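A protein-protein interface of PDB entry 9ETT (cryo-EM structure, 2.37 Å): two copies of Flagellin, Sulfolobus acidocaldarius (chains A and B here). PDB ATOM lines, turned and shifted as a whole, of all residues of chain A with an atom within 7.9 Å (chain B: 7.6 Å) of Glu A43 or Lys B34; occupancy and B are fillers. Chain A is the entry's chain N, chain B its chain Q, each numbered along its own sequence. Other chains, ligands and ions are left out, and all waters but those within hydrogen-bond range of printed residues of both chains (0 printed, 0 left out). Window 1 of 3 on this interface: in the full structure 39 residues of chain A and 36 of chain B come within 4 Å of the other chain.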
ATOM      1  N   THR A  37      21.648 -32.582   5.864  1.00  0.00           N
ATOM      2  CA  THR A  37      20.560 -33.185   6.624  1.00  0.00           C
ATOM      3  C   THR A  37      20.699 -32.877   8.117  1.00  0.00           C
ATOM      4  O   THR A  37      19.732 -32.470   8.755  1.00  0.00           O
ATOM      5  CB  THR A  37      20.499 -34.700   6.394  1.00  0.00           C
ATOM      6  OG1 THR A  37      20.346 -34.958   4.998  1.00  0.00           O
ATOM      7  CG2 THR A  37      19.371 -35.371   7.148  1.00  0.00           C
ATOM      8  N   THR A  38      21.909 -33.040   8.667  1.00  0.00           N
ATOM      9  CA  THR A  38      22.202 -32.783  10.071  1.00  0.00           C
ATOM     10  C   THR A  38      21.946 -31.319  10.434  1.00  0.00           C
ATOM     11  O   THR A  38      21.321 -31.049  11.451  1.00  0.00           O
ATOM     12  CB  THR A  38      23.636 -33.193  10.427  1.00  0.00           C
ATOM     13  OG1 THR A  38      23.735 -34.608  10.281  1.00  0.00           O
ATOM     14  CG2 THR A  38      24.043 -32.819  11.836  1.00  0.00           C
ATOM     15  N   ILE A  39      22.411 -30.375   9.607  1.00  0.00           N
ATOM     16  CA  ILE A  39      22.194 -28.947   9.813  1.00  0.00           C
ATOM     17  C   ILE A  39      20.693 -28.640   9.870  1.00  0.00           C
ATOM     18  O   ILE A  39      20.246 -27.928  10.764  1.00  0.00           O
ATOM     19  CB  ILE A  39      22.930 -28.111   8.742  1.00  0.00           C
ATOM     20  CG1 ILE A  39      24.450 -28.281   8.803  1.00  0.00           C
ATOM     21  CG2 ILE A  39      22.551 -26.643   8.873  1.00  0.00           C
ATOM     22  CD1 ILE A  39      25.165 -27.993   7.491  1.00  0.00           C
ATOM     23  N   ASN A  40      19.910 -29.211   8.949  1.00  0.00           N
ATOM     24  CA  ASN A  40      18.462 -29.086   8.954  1.00  0.00           C
ATOM     25  C   ASN A  40      17.850 -29.603  10.266  1.00  0.00           C
ATOM     26  O   ASN A  40      17.117 -28.876  10.935  1.00  0.00           O
ATOM     27  CB  ASN A  40      17.866 -29.748   7.715  1.00  0.00           C
ATOM     28  CG  ASN A  40      16.367 -29.562   7.685  1.00  0.00           C
ATOM     29  OD1 ASN A  40      15.888 -28.431   7.663  1.00  0.00           O
ATOM     30  ND2 ASN A  40      15.618 -30.651   7.752  1.00  0.00           N
ATOM     31  N   LYS A  41      18.195 -30.830  10.684  1.00  0.00           N
ATOM     32  CA  LYS A  41      17.694 -31.424  11.923  1.00  0.00           C
ATOM     33  C   LYS A  41      18.118 -30.637  13.168  1.00  0.00           C
ATOM     34  O   LYS A  41      17.371 -30.586  14.139  1.00  0.00           O
ATOM     35  CB  LYS A  41      18.091 -32.900  12.031  1.00  0.00           C
ATOM     36  CG  LYS A  41      17.391 -33.839  11.057  1.00  0.00           C
ATOM     37  CD  LYS A  41      15.908 -34.010  11.326  1.00  0.00           C
ATOM     38  CE  LYS A  41      15.121 -34.411  10.094  1.00  0.00           C
ATOM     39  NZ  LYS A  41      13.675 -34.128  10.247  1.00  0.00           N
ATOM     40  N   GLY A  42      19.301 -30.014  13.146  1.00  0.00           N
ATOM     41  CA  GLY A  42      19.773 -29.149  14.219  1.00  0.00           C
ATOM     42  C   GLY A  42      18.928 -27.884  14.359  1.00  0.00           C
ATOM     43  O   GLY A  42      18.531 -27.537  15.467  1.00  0.00           O
ATOM     44  N   GLU A  43      18.608 -27.227  13.237  1.00  0.00           N
ATOM     45  CA  GLU A  43      17.700 -26.087  13.242  1.00  0.00           C
ATOM     46  C   GLU A  43      16.302 -26.506  13.714  1.00  0.00           C
ATOM     47  O   GLU A  43      15.757 -25.872  14.610  1.00  0.00           O
ATOM     48  CB  GLU A  43      17.689 -25.379  11.886  1.00  0.00           C
ATOM     49  CG  GLU A  43      16.696 -24.225  11.809  1.00  0.00           C
ATOM     50  CD  GLU A  43      15.265 -24.588  11.432  1.00  0.00           C
ATOM     51  OE1 GLU A  43      15.067 -25.096  10.308  1.00  0.00           O
ATOM     52  OE2 GLU A  43      14.345 -24.352  12.252  1.00  0.00           O
ATOM     53  N   GLU A  44      15.744 -27.593  13.164  1.00  0.00           N
ATOM     54  CA  GLU A  44      14.446 -28.112  13.585  1.00  0.00           C
ATOM     55  C   GLU A  44      14.416 -28.394  15.092  1.00  0.00           C
ATOM     56  O   GLU A  44      13.431 -28.090  15.754  1.00  0.00           O
ATOM     57  CB  GLU A  44      14.097 -29.387  12.819  1.00  0.00           C
ATOM     58  CG  GLU A  44      13.743 -29.157  11.361  1.00  0.00           C
ATOM     59  CD  GLU A  44      13.488 -30.413  10.540  1.00  0.00           C
ATOM     60  OE1 GLU A  44      13.471 -31.517  11.124  1.00  0.00           O
ATOM     61  OE2 GLU A  44      13.298 -30.289   9.311  1.00  0.00           O
ATOM     62  N   THR A  45      15.504 -28.938  15.649  1.00  0.00           N
ATOM     63  CA  THR A  45      15.624 -29.218  17.076  1.00  0.00           C
ATOM     64  C   THR A  45      15.660 -27.937  17.913  1.00  0.00           C
ATOM     65  O   THR A  45      15.177 -27.926  19.040  1.00  0.00           O
ATOM     66  CB  THR A  45      16.852 -30.095  17.360  1.00  0.00           C
ATOM     67  OG1 THR A  45      16.616 -31.341  16.709  1.00  0.00           O
ATOM     68  CG2 THR A  45      17.115 -30.347  18.830  1.00  0.00           C
ATOM     69  N   ALA A  46      16.249 -26.859  17.385  1.00  0.00           N
ATOM     70  CA  ALA A  46      16.292 -25.573  18.065  1.00  0.00           C
ATOM     71  C   ALA A  46      14.968 -24.806  17.949  1.00  0.00           C
ATOM     72  O   ALA A  46      14.611 -24.077  18.871  1.00  0.00           O
ATOM     73  CB  ALA A  46      17.455 -24.771  17.547  1.00  0.00           C
ATOM     74  N   SER A  47      14.240 -24.956  16.830  1.00  0.00           N
ATOM     75  CA  SER A  47      13.005 -24.217  16.586  1.00  0.00           C
ATOM     76  C   SER A  47      11.771 -24.903  17.187  1.00  0.00           C
ATOM     77  O   SER A  47      10.960 -24.240  17.829  1.00  0.00           O
ATOM     78  CB  SER A  47      12.845 -23.868  15.121  1.00  0.00           C
ATOM     79  OG  SER A  47      12.721 -25.016  14.293  1.00  0.00           O
ATOM     80  N   THR A  48      11.624 -26.225  17.005  1.00  0.00           N
ATOM     81  CA  THR A  48      10.434 -26.936  17.472  1.00  0.00           C
ATOM     82  C   THR A  48      10.400 -27.042  19.002  1.00  0.00           C
ATOM     83  O   THR A  48      11.339 -27.525  19.629  1.00  0.00           O
ATOM     84  CB  THR A  48      10.257 -28.301  16.791  1.00  0.00           C
ATOM     85  OG1 THR A  48      11.398 -29.119  17.046  1.00  0.00           O
ATOM     86  CG2 THR A  48      10.095 -28.215  15.290  1.00  0.00           C
ATOM     87  N   VAL A  81       6.945 -20.460  15.683  1.00  0.00           N
ATOM     88  CA  VAL A  81       8.089 -20.615  14.781  1.00  0.00           C
ATOM     89  C   VAL A  81       7.962 -21.799  13.812  1.00  0.00           C
ATOM     90  O   VAL A  81       8.334 -21.667  12.641  1.00  0.00           O
ATOM     91  CB  VAL A  81       9.458 -20.568  15.490  1.00  0.00           C
ATOM     92  CG1 VAL A  81       9.648 -19.268  16.248  1.00  0.00           C
ATOM     93  CG2 VAL A  81       9.667 -21.741  16.435  1.00  0.00           C
ATOM     94  N   SER A  82       7.481 -22.959  14.297  1.00  0.00           N
ATOM     95  CA  SER A  82       7.424 -24.186  13.499  1.00  0.00           C
ATOM     96  C   SER A  82       6.421 -25.200  14.065  1.00  0.00           C
ATOM     97  O   SER A  82       5.997 -25.071  15.205  1.00  0.00           O
ATOM     98  CB  SER A  82       8.809 -24.786  13.292  1.00  0.00           C
ATOM     99  OG  SER A  82       9.480 -25.029  14.525  1.00  0.00           O
ATOM    100  N   ILE A 272      10.952 -34.665  17.762  1.00  0.00           N
ATOM    101  CA  ILE A 272      11.885 -33.620  17.353  1.00  0.00           C
ATOM    102  C   ILE A 272      11.656 -32.417  18.269  1.00  0.00           C
ATOM    103  O   ILE A 272      10.516 -32.097  18.590  1.00  0.00           O
ATOM    104  CB  ILE A 272      11.722 -33.250  15.856  1.00  0.00           C
ATOM    105  CG1 ILE A 272      11.864 -34.460  14.923  1.00  0.00           C
ATOM    106  CG2 ILE A 272      12.692 -32.147  15.452  1.00  0.00           C
ATOM    107  CD1 ILE A 272      11.444 -34.206  13.486  1.00  0.00           C
ATOM    108  N   GLY A 273      12.744 -31.756  18.693  1.00  0.00           N
ATOM    109  CA  GLY A 273      12.645 -30.548  19.501  1.00  0.00           C
ATOM    110  C   GLY A 273      12.611 -30.816  21.005  1.00  0.00           C
ATOM    111  O   GLY A 273      12.482 -31.957  21.452  1.00  0.00           O
ATOM    112  N   MET B  27      23.528 -24.048   2.825  1.00  0.00           N
ATOM    113  CA  MET B  27      22.906 -24.354   4.102  1.00  0.00           C
ATOM    114  C   MET B  27      23.081 -23.236   5.136  1.00  0.00           C
ATOM    115  O   MET B  27      22.187 -23.029   5.950  1.00  0.00           O
ATOM    116  CB  MET B  27      23.375 -25.707   4.625  1.00  0.00           C
ATOM    117  CG  MET B  27      22.292 -26.410   5.399  1.00  0.00           C
ATOM    118  SD  MET B  27      20.801 -26.780   4.436  1.00  0.00           S
ATOM    119  CE  MET B  27      19.588 -26.869   5.753  1.00  0.00           C
ATOM    120  N   GLY B  28      24.174 -22.461   5.060  1.00  0.00           N
ATOM    121  CA  GLY B  28      24.341 -21.225   5.813  1.00  0.00           C
ATOM    122  C   GLY B  28      23.322 -20.155   5.414  1.00  0.00           C
ATOM    123  O   GLY B  28      22.705 -19.545   6.279  1.00  0.00           O
ATOM    124  N   LEU B  29      23.107 -19.952   4.107  1.00  0.00           N
ATOM    125  CA  LEU B  29      22.060 -19.059   3.624  1.00  0.00           C
ATOM    126  C   LEU B  29      20.685 -19.493   4.142  1.00  0.00           C
ATOM    127  O   LEU B  29      19.926 -18.661   4.630  1.00  0.00           O
ATOM    128  CB  LEU B  29      22.112 -18.978   2.095  1.00  0.00           C
ATOM    129  CG  LEU B  29      23.303 -18.212   1.522  1.00  0.00           C
ATOM    130  CD1 LEU B  29      23.564 -18.613   0.080  1.00  0.00           C
ATOM    131  CD2 LEU B  29      23.101 -16.709   1.632  1.00  0.00           C
ATOM    132  N   PHE B  30      20.388 -20.797   4.103  1.00  0.00           N
ATOM    133  CA  PHE B  30      19.159 -21.351   4.650  1.00  0.00           C
ATOM    134  C   PHE B  30      19.013 -21.052   6.147  1.00  0.00           C
ATOM    135  O   PHE B  30      18.050 -20.395   6.547  1.00  0.00           O
ATOM    136  CB  PHE B  30      19.086 -22.845   4.337  1.00  0.00           C
ATOM    137  CG  PHE B  30      17.818 -23.542   4.773  1.00  0.00           C
ATOM    138  CD1 PHE B  30      17.644 -23.970   6.086  1.00  0.00           C
ATOM    139  CD2 PHE B  30      16.800 -23.793   3.862  1.00  0.00           C
ATOM    140  CE1 PHE B  30      16.486 -24.635   6.472  1.00  0.00           C
ATOM    141  CE2 PHE B  30      15.637 -24.449   4.250  1.00  0.00           C
ATOM    142  CZ  PHE B  30      15.486 -24.871   5.552  1.00  0.00           C
ATOM    143  N   VAL B  31      19.966 -21.497   6.979  1.00  0.00           N
ATOM    144  CA  VAL B  31      19.841 -21.413   8.433  1.00  0.00           C
ATOM    145  C   VAL B  31      19.826 -19.962   8.921  1.00  0.00           C
ATOM    146  O   VAL B  31      19.053 -19.628   9.815  1.00  0.00           O
ATOM    147  CB  VAL B  31      20.899 -22.268   9.159  1.00  0.00           C
ATOM    148  CG1 VAL B  31      20.942 -22.018  10.664  1.00  0.00           C
ATOM    149  CG2 VAL B  31      20.650 -23.737   8.894  1.00  0.00           C
ATOM    150  N   THR B  32      20.626 -19.079   8.319  1.00  0.00           N
ATOM    151  CA  THR B  32      20.616 -17.667   8.689  1.00  0.00           C
ATOM    152  C   THR B  32      19.272 -17.010   8.379  1.00  0.00           C
ATOM    153  O   THR B  32      18.799 -16.189   9.155  1.00  0.00           O
ATOM    154  CB  THR B  32      21.792 -16.893   8.084  1.00  0.00           C
ATOM    155  OG1 THR B  32      21.745 -17.022   6.663  1.00  0.00           O
ATOM    156  CG2 THR B  32      23.127 -17.375   8.602  1.00  0.00           C
ATOM    157  N   GLN B  33      18.590 -17.434   7.314  1.00  0.00           N
ATOM    158  CA  GLN B  33      17.243 -16.953   7.034  1.00  0.00           C
ATOM    159  C   GLN B  33      16.190 -17.527   7.998  1.00  0.00           C
ATOM    160  O   GLN B  33      15.274 -16.810   8.407  1.00  0.00           O
ATOM    161  CB  GLN B  33      16.940 -17.238   5.576  1.00  0.00           C
ATOM    162  CG  GLN B  33      15.716 -16.482   5.094  1.00  0.00           C
ATOM    163  CD  GLN B  33      15.269 -16.910   3.719  1.00  0.00           C
ATOM    164  OE1 GLN B  33      14.114 -17.279   3.511  1.00  0.00           O
ATOM    165  NE2 GLN B  33      16.182 -16.857   2.761  1.00  0.00           N
ATOM    166  N   LYS B  34      16.325 -18.798   8.410  1.00  0.00           N
ATOM    167  CA  LYS B  34      15.522 -19.374   9.490  1.00  0.00           C
ATOM    168  C   LYS B  34      15.709 -18.584  10.791  1.00  0.00           C
ATOM    169  O   LYS B  34      14.737 -18.320  11.497  1.00  0.00           O
ATOM    170  CB  LYS B  34      15.818 -20.866   9.690  1.00  0.00           C
ATOM    171  CG  LYS B  34      15.574 -21.784   8.493  1.00  0.00           C
ATOM    172  CD  LYS B  34      14.123 -21.907   8.042  1.00  0.00           C
ATOM    173  CE  LYS B  34      13.222 -22.615   9.030  1.00  0.00           C
ATOM    174  NZ  LYS B  34      11.849 -22.769   8.493  1.00  0.00           N
ATOM    175  N   ALA B  35      16.946 -18.158  11.086  1.00  0.00           N
ATOM    176  CA  ALA B  35      17.254 -17.285  12.210  1.00  0.00           C
ATOM    177  C   ALA B  35      16.572 -15.918  12.063  1.00  0.00           C
ATOM    178  O   ALA B  35      15.872 -15.508  12.983  1.00  0.00           O
ATOM    179  CB  ALA B  35      18.748 -17.189  12.420  1.00  0.00           C
ATOM    180  N   LYS B  36      16.686 -15.254  10.899  1.00  0.00           N
ATOM    181  CA  LYS B  36      16.006 -13.990  10.614  1.00  0.00           C
ATOM    182  C   LYS B  36      14.505 -14.079  10.916  1.00  0.00           C
ATOM    183  O   LYS B  36      13.969 -13.266  11.675  1.00  0.00           O
ATOM    184  CB  LYS B  36      16.281 -13.561   9.169  1.00  0.00           C
ATOM    185  CG  LYS B  36      15.754 -12.177   8.816  1.00  0.00           C
ATOM    186  CD  LYS B  36      15.834 -11.836   7.343  1.00  0.00           C
ATOM    187  CE  LYS B  36      15.548 -10.379   7.032  1.00  0.00           C
ATOM    188  NZ  LYS B  36      14.148 -10.002   7.346  1.00  0.00           N
ATOM    189  N   THR B  37      13.843 -15.098  10.351  1.00  0.00           N
ATOM    190  CA  THR B  37      12.419 -15.354  10.537  1.00  0.00           C
ATOM    191  C   THR B  37      12.091 -15.571  12.015  1.00  0.00           C
ATOM    192  O   THR B  37      11.145 -14.981  12.529  1.00  0.00           O
ATOM    193  CB  THR B  37      11.964 -16.560   9.704  1.00  0.00           C
ATOM    194  OG1 THR B  37      12.260 -16.323   8.328  1.00  0.00           O
ATOM    195  CG2 THR B  37      10.486 -16.858   9.848  1.00  0.00           C
ATOM    196  N   THR B  38      12.892 -16.391  12.708  1.00  0.00           N
ATOM    197  CA  THR B  38      12.713 -16.695  14.122  1.00  0.00           C
ATOM    198  C   THR B  38      12.828 -15.434  14.979  1.00  0.00           C
ATOM    199  O   THR B  38      11.996 -15.216  15.850  1.00  0.00           O
ATOM    200  CB  THR B  38      13.700 -17.770  14.593  1.00  0.00           C
ATOM    201  OG1 THR B  38      13.382 -18.983  13.913  1.00  0.00           O
ATOM    202  CG2 THR B  38      13.648 -18.020  16.086  1.00  0.00           C
ATOM    203  N   ILE B  39      13.842 -14.596  14.734  1.00  0.00           N
ATOM    204  CA  ILE B  39      14.037 -13.339  15.447  1.00  0.00           C
ATOM    205  C   ILE B  39      12.808 -12.438  15.286  1.00  0.00           C
ATOM    206  O   ILE B  39      12.318 -11.886  16.267  1.00  0.00           O
ATOM    207  CB  ILE B  39      15.346 -12.645  15.006  1.00  0.00           C
ATOM    208  CG1 ILE B  39      16.590 -13.475  15.337  1.00  0.00           C
ATOM    209  CG2 ILE B  39      15.442 -11.265  15.637  1.00  0.00           C
ATOM    210  CD1 ILE B  39      17.796 -13.179  14.461  1.00  0.00           C
ATOM    211  N   ASN B  40      12.280 -12.326  14.063  1.00  0.00           N
ATOM    212  CA  ASN B  40      11.055 -11.592  13.794  1.00  0.00           C
ATOM    213  C   ASN B  40       9.872 -12.137  14.609  1.00  0.00           C
ATOM    214  O   ASN B  40       9.221 -11.386  15.332  1.00  0.00           O
ATOM    215  CB  ASN B  40      10.779 -11.548  12.293  1.00  0.00           C
ATOM    216  CG  ASN B  40       9.541 -10.732  12.007  1.00  0.00           C
ATOM    217  OD1 ASN B  40       9.492  -9.550  12.339  1.00  0.00           O
ATOM    218  ND2 ASN B  40       8.514 -11.358  11.455  1.00  0.00           N
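4 positions are printed for both chains.
Of the 14 printed residues of chain B, 3 touch a printed residue of chain A.
Printed residues of chain B that touch a printed residue of chain A: Met B27, Val B31 and Lys B34.
Along chain B the printed residues that touch a printed residue of chain A span positions 27 to 34.
Printed residues of chain A that touch a printed residue of chain B: Ile A39, Asn A40 and Glu A43.
Along chain A the printed residues that touch a printed residue of chain B span positions 39 to 43.
Among the printed residues, no Asp or Glu carboxylate lies within 4 Å of a Lys or Arg side-chain nitrogen of the other chain.
Among the printed residues, merely in contact across the chains: Glu A43 with Lys B34 (3.3 Å), Ile A39 with Val B31 (3.5 Å), Ile A39 with Met B27 (3.5 Å) and Asn A40 with Met B27 (3.9 Å).
Glu A43 touches one residue of chain B.
Of chain A, only Glu A43 comes within 4 Å of Lys B34.
No residue of chain A comes within 4 Å of Ala B35.
Of the printed residues of chain B, Asn A40 touches Met B27.
Printed residues of chain B within 4 Å of Ile A39: Met B27 and Val B31.
Gly B28 touches none of the printed residues of chain A.
Thr B32 touches none of the printed residues of chain A.
The nearest residue of chain B that does not touch Glu A43 is Phe B30 (4.1 Å).
The nearest printed residue of chain B that does not touch Asn A40 is Phe B30 (4.02 Å).
The side-chain carboxylate (OE2) of Glu A44 is in hydrogen-bond range of the side-chain amide nitrogen (ND2) of Asn A40 (2.8 Å).
OE2 of Glu A43 lies within hydrogen-bond range of OG of Ser A47, at 2.7 Å.
The side-chain hydroxyl (OG1) of Thr B38 lies within hydrogen-bond range of the backbone carbonyl oxygen (O) of Lys B34, 2.8 Å away.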
